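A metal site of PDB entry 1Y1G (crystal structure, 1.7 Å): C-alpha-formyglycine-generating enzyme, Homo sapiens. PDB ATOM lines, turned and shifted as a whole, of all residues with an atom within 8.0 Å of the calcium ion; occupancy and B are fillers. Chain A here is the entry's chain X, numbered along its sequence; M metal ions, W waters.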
ATOM      1  N   TYR A  57     -29.348  11.036  23.306  1.00  0.00           N
ATOM      2  CA  TYR A  57     -28.340   9.987  23.457  1.00  0.00           C
ATOM      3  C   TYR A  57     -26.941  10.578  23.617  1.00  0.00           C
ATOM      4  O   TYR A  57     -26.635  11.658  23.089  1.00  0.00           O
ATOM      5  CB  TYR A  57     -28.311   9.138  22.177  1.00  0.00           C
ATOM      6  CG  TYR A  57     -29.674   8.652  21.748  1.00  0.00           C
ATOM      7  CD1 TYR A  57     -30.351   7.706  22.492  1.00  0.00           C
ATOM      8  CD2 TYR A  57     -30.289   9.162  20.610  1.00  0.00           C
ATOM      9  CE1 TYR A  57     -31.601   7.229  22.093  1.00  0.00           C
ATOM     10  CE2 TYR A  57     -31.537   8.715  20.209  1.00  0.00           C
ATOM     11  CZ  TYR A  57     -32.175   7.737  20.957  1.00  0.00           C
ATOM     12  OH  TYR A  57     -33.421   7.277  20.561  1.00  0.00           O
ATOM     13  N   GLU A  58     -26.100   9.866  24.356  1.00  0.00           N
ATOM     14  CA  GLU A  58     -24.653  10.095  24.282  1.00  0.00           C
ATOM     15  C   GLU A  58     -24.271  10.030  22.795  1.00  0.00           C
ATOM     16  O   GLU A  58     -24.888   9.311  22.029  1.00  0.00           O
ATOM     17  CB  GLU A  58     -23.908   8.994  25.033  1.00  0.00           C
ATOM     18  CG  GLU A  58     -24.204   8.944  26.535  1.00  0.00           C
ATOM     19  CD  GLU A  58     -23.972   7.565  27.177  1.00  0.00           C
ATOM     20  OE1 GLU A  58     -24.189   6.555  26.488  1.00  0.00           O
ATOM     21  OE2 GLU A  58     -23.571   7.526  28.370  1.00  0.00           O
ATOM     22  N   PRO A 133     -21.480   4.523  22.881  1.00  0.00           N
ATOM     23  CA  PRO A 133     -20.978   5.895  23.012  1.00  0.00           C
ATOM     24  C   PRO A 133     -19.519   6.002  22.590  1.00  0.00           C
ATOM     25  O   PRO A 133     -18.718   5.104  22.853  1.00  0.00           O
ATOM     26  CB  PRO A 133     -21.115   6.196  24.522  1.00  0.00           C
ATOM     27  CG  PRO A 133     -21.130   4.870  25.158  1.00  0.00           C
ATOM     28  CD  PRO A 133     -21.850   3.973  24.185  1.00  0.00           C
ATOM     29  N   TRP A 159     -27.168  20.268  32.424  1.00  0.00           N
ATOM     30  CA  TRP A 159     -26.986  18.819  32.441  1.00  0.00           C
ATOM     31  C   TRP A 159     -27.738  18.217  33.629  1.00  0.00           C
ATOM     32  O   TRP A 159     -28.505  17.261  33.484  1.00  0.00           O
ATOM     33  CB  TRP A 159     -25.486  18.445  32.455  1.00  0.00           C
ATOM     34  CG  TRP A 159     -25.259  16.981  32.229  1.00  0.00           C
ATOM     35  CD1 TRP A 159     -24.871  16.373  31.065  1.00  0.00           C
ATOM     36  CD2 TRP A 159     -25.429  15.934  33.186  1.00  0.00           C
ATOM     37  NE1 TRP A 159     -24.780  15.013  31.256  1.00  0.00           N
ATOM     38  CE2 TRP A 159     -25.139  14.715  32.537  1.00  0.00           C
ATOM     39  CE3 TRP A 159     -25.813  15.900  34.521  1.00  0.00           C
ATOM     40  CZ2 TRP A 159     -25.220  13.505  33.194  1.00  0.00           C
ATOM     41  CZ3 TRP A 159     -25.922  14.693  35.155  1.00  0.00           C
ATOM     42  CH2 TRP A 159     -25.617  13.505  34.483  1.00  0.00           C
ATOM     43  N   ASN A 187     -26.568   1.485  33.156  1.00  0.00           N
ATOM     44  CA  ASN A 187     -25.417   0.619  33.014  1.00  0.00           C
ATOM     45  C   ASN A 187     -24.295   1.070  33.960  1.00  0.00           C
ATOM     46  O   ASN A 187     -23.551   1.995  33.648  1.00  0.00           O
ATOM     47  CB  ASN A 187     -24.942   0.614  31.570  1.00  0.00           C
ATOM     48  CG  ASN A 187     -23.719  -0.259  31.352  1.00  0.00           C
ATOM     49  OD1 ASN A 187     -23.434  -1.169  32.157  1.00  0.00           O
ATOM     50  ND2 ASN A 187     -22.994   0.000  30.252  1.00  0.00           N
ATOM     51  N   TYR A 220     -31.579   9.129  27.415  1.00  0.00           N
ATOM     52  CA  TYR A 220     -31.104   7.764  27.635  1.00  0.00           C
ATOM     53  C   TYR A 220     -29.711   7.828  28.242  1.00  0.00           C
ATOM     54  O   TYR A 220     -28.874   8.631  27.808  1.00  0.00           O
ATOM     55  CB  TYR A 220     -31.048   7.003  26.298  1.00  0.00           C
ATOM     56  CG  TYR A 220     -32.412   6.710  25.743  1.00  0.00           C
ATOM     57  CD1 TYR A 220     -33.131   7.698  25.105  1.00  0.00           C
ATOM     58  CD2 TYR A 220     -32.996   5.478  25.930  1.00  0.00           C
ATOM     59  CE1 TYR A 220     -34.387   7.462  24.622  1.00  0.00           C
ATOM     60  CE2 TYR A 220     -34.274   5.206  25.440  1.00  0.00           C
ATOM     61  CZ  TYR A 220     -34.968   6.219  24.800  1.00  0.00           C
ATOM     62  OH  TYR A 220     -36.236   5.957  24.312  1.00  0.00           O
ATOM     63  N   ASN A 221     -29.445   6.952  29.215  1.00  0.00           N
ATOM     64  CA  ASN A 221     -28.097   6.794  29.777  1.00  0.00           C
ATOM     65  C   ASN A 221     -27.480   8.068  30.323  1.00  0.00           C
ATOM     66  O   ASN A 221     -26.270   8.271  30.275  1.00  0.00           O
ATOM     67  CB  ASN A 221     -27.188   6.101  28.774  1.00  0.00           C
ATOM     68  CG  ASN A 221     -27.697   4.732  28.420  1.00  0.00           C
ATOM     69  OD1 ASN A 221     -27.814   3.859  29.279  1.00  0.00           O
ATOM     70  ND2 ASN A 221     -28.103   4.563  27.165  1.00  0.00           N
ATOM     71  N   ILE A 222     -28.334   8.913  30.888  1.00  0.00           N
ATOM     72  CA  ILE A 222     -27.864  10.181  31.460  1.00  0.00           C
ATOM     73  C   ILE A 222     -27.062   9.909  32.740  1.00  0.00           C
ATOM     74  O   ILE A 222     -26.070  10.581  33.011  1.00  0.00           O
ATOM     75  CB  ILE A 222     -28.999  11.201  31.621  1.00  0.00           C
ATOM     76  CG1 ILE A 222     -28.413  12.613  31.885  1.00  0.00           C
ATOM     77  CG2 ILE A 222     -29.963  10.837  32.698  1.00  0.00           C
ATOM     78  CD1 ILE A 222     -27.826  13.291  30.707  1.00  0.00           C
ATOM     79  N   VAL A 223     -27.437   8.889  33.518  1.00  0.00           N
ATOM     80  CA  VAL A 223     -26.474   8.304  34.463  1.00  0.00           C
ATOM     81  C   VAL A 223     -25.985   6.945  33.925  1.00  0.00           C
ATOM     82  O   VAL A 223     -26.720   6.229  33.238  1.00  0.00           O
ATOM     83  CB  VAL A 223     -26.965   8.183  35.900  1.00  0.00           C
ATOM     84  CG1 VAL A 223     -27.334   9.534  36.422  1.00  0.00           C
ATOM     85  CG2 VAL A 223     -28.121   7.194  36.057  1.00  0.00           C
ATOM     86  N   GLY A 224     -24.739   6.615  34.239  1.00  0.00           N
ATOM     87  CA  GLY A 224     -24.129   5.396  33.765  1.00  0.00           C
ATOM     88  C   GLY A 224     -23.732   5.415  32.293  1.00  0.00           C
ATOM     89  O   GLY A 224     -23.870   6.432  31.578  1.00  0.00           O
ATOM     90  N   ASN A 225     -23.239   4.261  31.845  1.00  0.00           N
ATOM     91  CA  ASN A 225     -22.715   4.069  30.496  1.00  0.00           C
ATOM     92  C   ASN A 225     -21.423   4.856  30.316  1.00  0.00           C
ATOM     93  O   ASN A 225     -20.400   4.413  30.850  1.00  0.00           O
ATOM     94  CB  ASN A 225     -23.773   4.297  29.410  1.00  0.00           C
ATOM     95  CG  ASN A 225     -23.617   3.322  28.239  1.00  0.00           C
ATOM     96  OD1 ASN A 225     -23.205   2.190  28.450  1.00  0.00           O
ATOM     97  ND2 ASN A 225     -23.958   3.758  27.026  1.00  0.00           N
ATOM     98  N   ALA A 226     -21.437   6.003  29.643  1.00  0.00           N
ATOM     99  CA  ALA A 226     -20.247   6.860  29.590  1.00  0.00           C
ATOM    100  C   ALA A 226     -20.463   8.054  30.519  1.00  0.00           C
ATOM    101  O   ALA A 226     -21.576   8.586  30.582  1.00  0.00           O
ATOM    102  CB  ALA A 226     -19.972   7.357  28.178  1.00  0.00           C
ATOM    103  N   TRP A 227     -19.406   8.479  31.228  1.00  0.00           N
ATOM    104  CA  TRP A 227     -19.357   9.810  31.829  1.00  0.00           C
ATOM    105  C   TRP A 227     -19.589  10.870  30.750  1.00  0.00           C
ATOM    106  O   TRP A 227     -19.368  10.619  29.554  1.00  0.00           O
ATOM    107  CB  TRP A 227     -17.969  10.106  32.444  1.00  0.00           C
ATOM    108  CG  TRP A 227     -17.702   9.611  33.801  1.00  0.00           C
ATOM    109  CD1 TRP A 227     -17.054   8.471  34.152  1.00  0.00           C
ATOM    110  CD2 TRP A 227     -18.012  10.291  35.023  1.00  0.00           C
ATOM    111  NE1 TRP A 227     -16.977   8.377  35.533  1.00  0.00           N
ATOM    112  CE2 TRP A 227     -17.560   9.489  36.091  1.00  0.00           C
ATOM    113  CE3 TRP A 227     -18.647  11.504  35.315  1.00  0.00           C
ATOM    114  CZ2 TRP A 227     -17.717   9.857  37.431  1.00  0.00           C
ATOM    115  CZ3 TRP A 227     -18.831  11.861  36.652  1.00  0.00           C
ATOM    116  CH2 TRP A 227     -18.334  11.050  37.685  1.00  0.00           C
ATOM    117  N   GLU A 228     -20.019  12.061  31.158  1.00  0.00           N
ATOM    118  CA  GLU A 228     -20.350  13.098  30.184  1.00  0.00           C
ATOM    119  C   GLU A 228     -19.744  14.453  30.512  1.00  0.00           C
ATOM    120  O   GLU A 228     -19.937  15.008  31.600  1.00  0.00           O
ATOM    121  CB  GLU A 228     -21.878  13.176  30.051  1.00  0.00           C
ATOM    122  CG  GLU A 228     -22.454  11.825  29.703  1.00  0.00           C
ATOM    123  CD  GLU A 228     -23.972  11.778  29.522  1.00  0.00           C
ATOM    124  OE1 GLU A 228     -24.619  12.825  29.399  1.00  0.00           O
ATOM    125  OE2 GLU A 228     -24.502  10.637  29.461  1.00  0.00           O
ATOM    126  N   LYS A 258     -20.078  14.654  34.412  1.00  0.00           N
ATOM    127  CA  LYS A 258     -21.262  14.250  35.161  1.00  0.00           C
ATOM    128  C   LYS A 258     -21.741  12.854  34.791  1.00  0.00           C
ATOM    129  O   LYS A 258     -21.506  12.342  33.683  1.00  0.00           O
ATOM    130  CB  LYS A 258     -22.434  15.233  34.912  1.00  0.00           C
ATOM    131  CG  LYS A 258     -22.186  16.688  35.365  1.00  0.00           C
ATOM    132  CD  LYS A 258     -22.323  16.905  36.875  1.00  0.00           C
ATOM    133  CE  LYS A 258     -23.758  17.158  37.291  1.00  0.00           C
ATOM    134  NZ  LYS A 258     -23.871  17.514  38.761  1.00  0.00           N
ATOM    135  N   GLY A 259     -22.454  12.273  35.747  1.00  0.00           N
ATOM    136  CA  GLY A 259     -23.358  11.167  35.477  1.00  0.00           C
ATOM    137  C   GLY A 259     -22.840   9.771  35.723  1.00  0.00           C
ATOM    138  O   GLY A 259     -23.627   8.819  35.749  1.00  0.00           O
ATOM    139  N   GLY A 260     -21.524   9.609  35.881  1.00  0.00           N
ATOM    140  CA  GLY A 260     -20.978   8.268  36.124  1.00  0.00           C
ATOM    141  C   GLY A 260     -21.058   7.377  34.902  1.00  0.00           C
ATOM    142  O   GLY A 260     -21.474   7.808  33.835  1.00  0.00           O
ATOM    143  N   SER A 261     -20.601   6.125  35.067  1.00  0.00           N
ATOM    144  CA  SER A 261     -20.322   5.236  33.960  1.00  0.00           C
ATOM    145  C   SER A 261     -20.539   3.771  34.304  1.00  0.00           C
ATOM    146  O   SER A 261     -20.899   3.445  35.436  1.00  0.00           O
ATOM    147  CB  SER A 261     -18.889   5.420  33.492  1.00  0.00           C
ATOM    148  OG  SER A 261     -17.978   4.815  34.402  1.00  0.00           O
ATOM    149  N   TYR A 262     -20.293   2.907  33.328  1.00  0.00           N
ATOM    150  CA  TYR A 262     -20.339   1.442  33.524  1.00  0.00           C
ATOM    151  C   TYR A 262     -19.388   0.916  34.585  1.00  0.00           C
ATOM    152  O   TYR A 262     -19.498  -0.241  34.998  1.00  0.00           O
ATOM    153  CB  TYR A 262     -20.060   0.743  32.203  1.00  0.00           C
ATOM    154  CG  TYR A 262     -18.664   0.913  31.651  1.00  0.00           C
ATOM    155  CD1 TYR A 262     -18.378   1.867  30.657  1.00  0.00           C
ATOM    156  CD2 TYR A 262     -17.643   0.074  32.058  1.00  0.00           C
ATOM    157  CE1 TYR A 262     -17.100   1.991  30.119  1.00  0.00           C
ATOM    158  CE2 TYR A 262     -16.368   0.182  31.517  1.00  0.00           C
ATOM    159  CZ  TYR A 262     -16.092   1.136  30.566  1.00  0.00           C
ATOM    160  OH  TYR A 262     -14.819   1.212  30.042  1.00  0.00           O
ATOM    161  N   ASN A 288     -14.025   5.453  29.684  1.00  0.00           N
ATOM    162  CA  ASN A 288     -15.354   5.524  30.285  1.00  0.00           C
ATOM    163  C   ASN A 288     -15.978   6.914  30.189  1.00  0.00           C
ATOM    164  O   ASN A 288     -16.926   7.206  30.891  1.00  0.00           O
ATOM    165  CB  ASN A 288     -15.312   5.067  31.742  1.00  0.00           C
ATOM    166  CG  ASN A 288     -14.600   6.034  32.625  1.00  0.00           C
ATOM    167  OD1 ASN A 288     -13.868   6.894  32.151  1.00  0.00           O
ATOM    168  ND2 ASN A 288     -14.832   5.926  33.943  1.00  0.00           N
ATOM    169  N   GLY A 290     -17.354  10.081  27.714  1.00  0.00           N
ATOM    170  CA  GLY A 290     -17.891  10.543  26.429  1.00  0.00           C
ATOM    171  C   GLY A 290     -18.621  11.863  26.690  1.00  0.00           C
ATOM    172  O   GLY A 290     -18.231  12.673  27.557  1.00  0.00           O
ATOM    173  N   PHE A 291     -19.705  12.088  25.931  1.00  0.00           N
ATOM    174  CA  PHE A 291     -20.435  13.342  26.023  1.00  0.00           C
ATOM    175  C   PHE A 291     -21.741  13.296  25.244  1.00  0.00           C
ATOM    176  O   PHE A 291     -21.944  12.426  24.421  1.00  0.00           O
ATOM    177  CB  PHE A 291     -19.609  14.533  25.528  1.00  0.00           C
ATOM    178  CG  PHE A 291     -19.310  14.513  24.043  1.00  0.00           C
ATOM    179  CD1 PHE A 291     -19.977  15.352  23.169  1.00  0.00           C
ATOM    180  CD2 PHE A 291     -18.345  13.686  23.531  1.00  0.00           C
ATOM    181  CE1 PHE A 291     -19.679  15.347  21.816  1.00  0.00           C
ATOM    182  CE2 PHE A 291     -18.072  13.657  22.165  1.00  0.00           C
ATOM    183  CZ  PHE A 291     -18.729  14.491  21.312  1.00  0.00           C
ATOM    184  N   ARG A 292     -22.587  14.294  25.497  1.00  0.00           N
ATOM    185  CA  ARG A 292     -23.712  14.589  24.618  1.00  0.00           C
ATOM    186  C   ARG A 292     -23.793  16.108  24.460  1.00  0.00           C
ATOM    187  O   ARG A 292     -23.230  16.856  25.256  1.00  0.00           O
ATOM    188  CB  ARG A 292     -25.041  14.050  25.166  1.00  0.00           C
ATOM    189  CG  ARG A 292     -25.627  14.862  26.300  1.00  0.00           C
ATOM    190  CD  ARG A 292     -26.915  14.211  26.825  1.00  0.00           C
ATOM    191  NE  ARG A 292     -26.625  12.942  27.494  1.00  0.00           N
ATOM    192  CZ  ARG A 292     -27.378  11.850  27.429  1.00  0.00           C
ATOM    193  NH1 ARG A 292     -28.469  11.827  26.702  1.00  0.00           N
ATOM    194  NH2 ARG A 292     -27.022  10.771  28.096  1.00  0.00           N
HETATM  195 CA    CA M   1     -23.930   8.538  30.388  1.00  0.00          CA
HETATM  196  O   HOH W   1     -23.570   9.524  32.537  1.00  0.00           O
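Merely in contact with the calcium ion: Ile 222 (3.95 Å).
Six residues have an atom within 4 Å of the calcium ion: Glu 58, Asn 221, Ile 222, Gly 224, Ala 226 and Glu 228.
The nearest printed residue that does not touch the calcium ion is Gly 260 (4.3 Å).
The calcium ion is bound by OE2 of Glu 58, O of Asn 221, O of Ala 226, OE2 of Glu 228, water W1 and O of Gly 224.
OE1 of Glu 228 lies within salt-bridge range of NE of Arg 292 (2.8 Å).
The backbone carbonyl oxygen (O) of Gly 259 is in hydrogen-bond range of the backbone NH (N) of Gly 224 (2.9 Å).
N of Lys 258 is in hydrogen-bond range of O of Glu 228, 2.8 Å away.
The side-chain carboxylate (OE1) of Glu 228 lies within hydrogen-bond range of the indole nitrogen (NE1) of Trp 159.
O of Asn 221 sits close to NH2 of Arg 292 (3.4 Å).
The backbone NH of Gly 224 lies within hydrogen-bond range of the backbone carbonyl oxygen of Gly 260 (3.5 Å).
The side-chain carboxylate of Glu 58 is in hydrogen-bond range of the side-chain amide nitrogen of Asn 225, at 2.9 Å.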
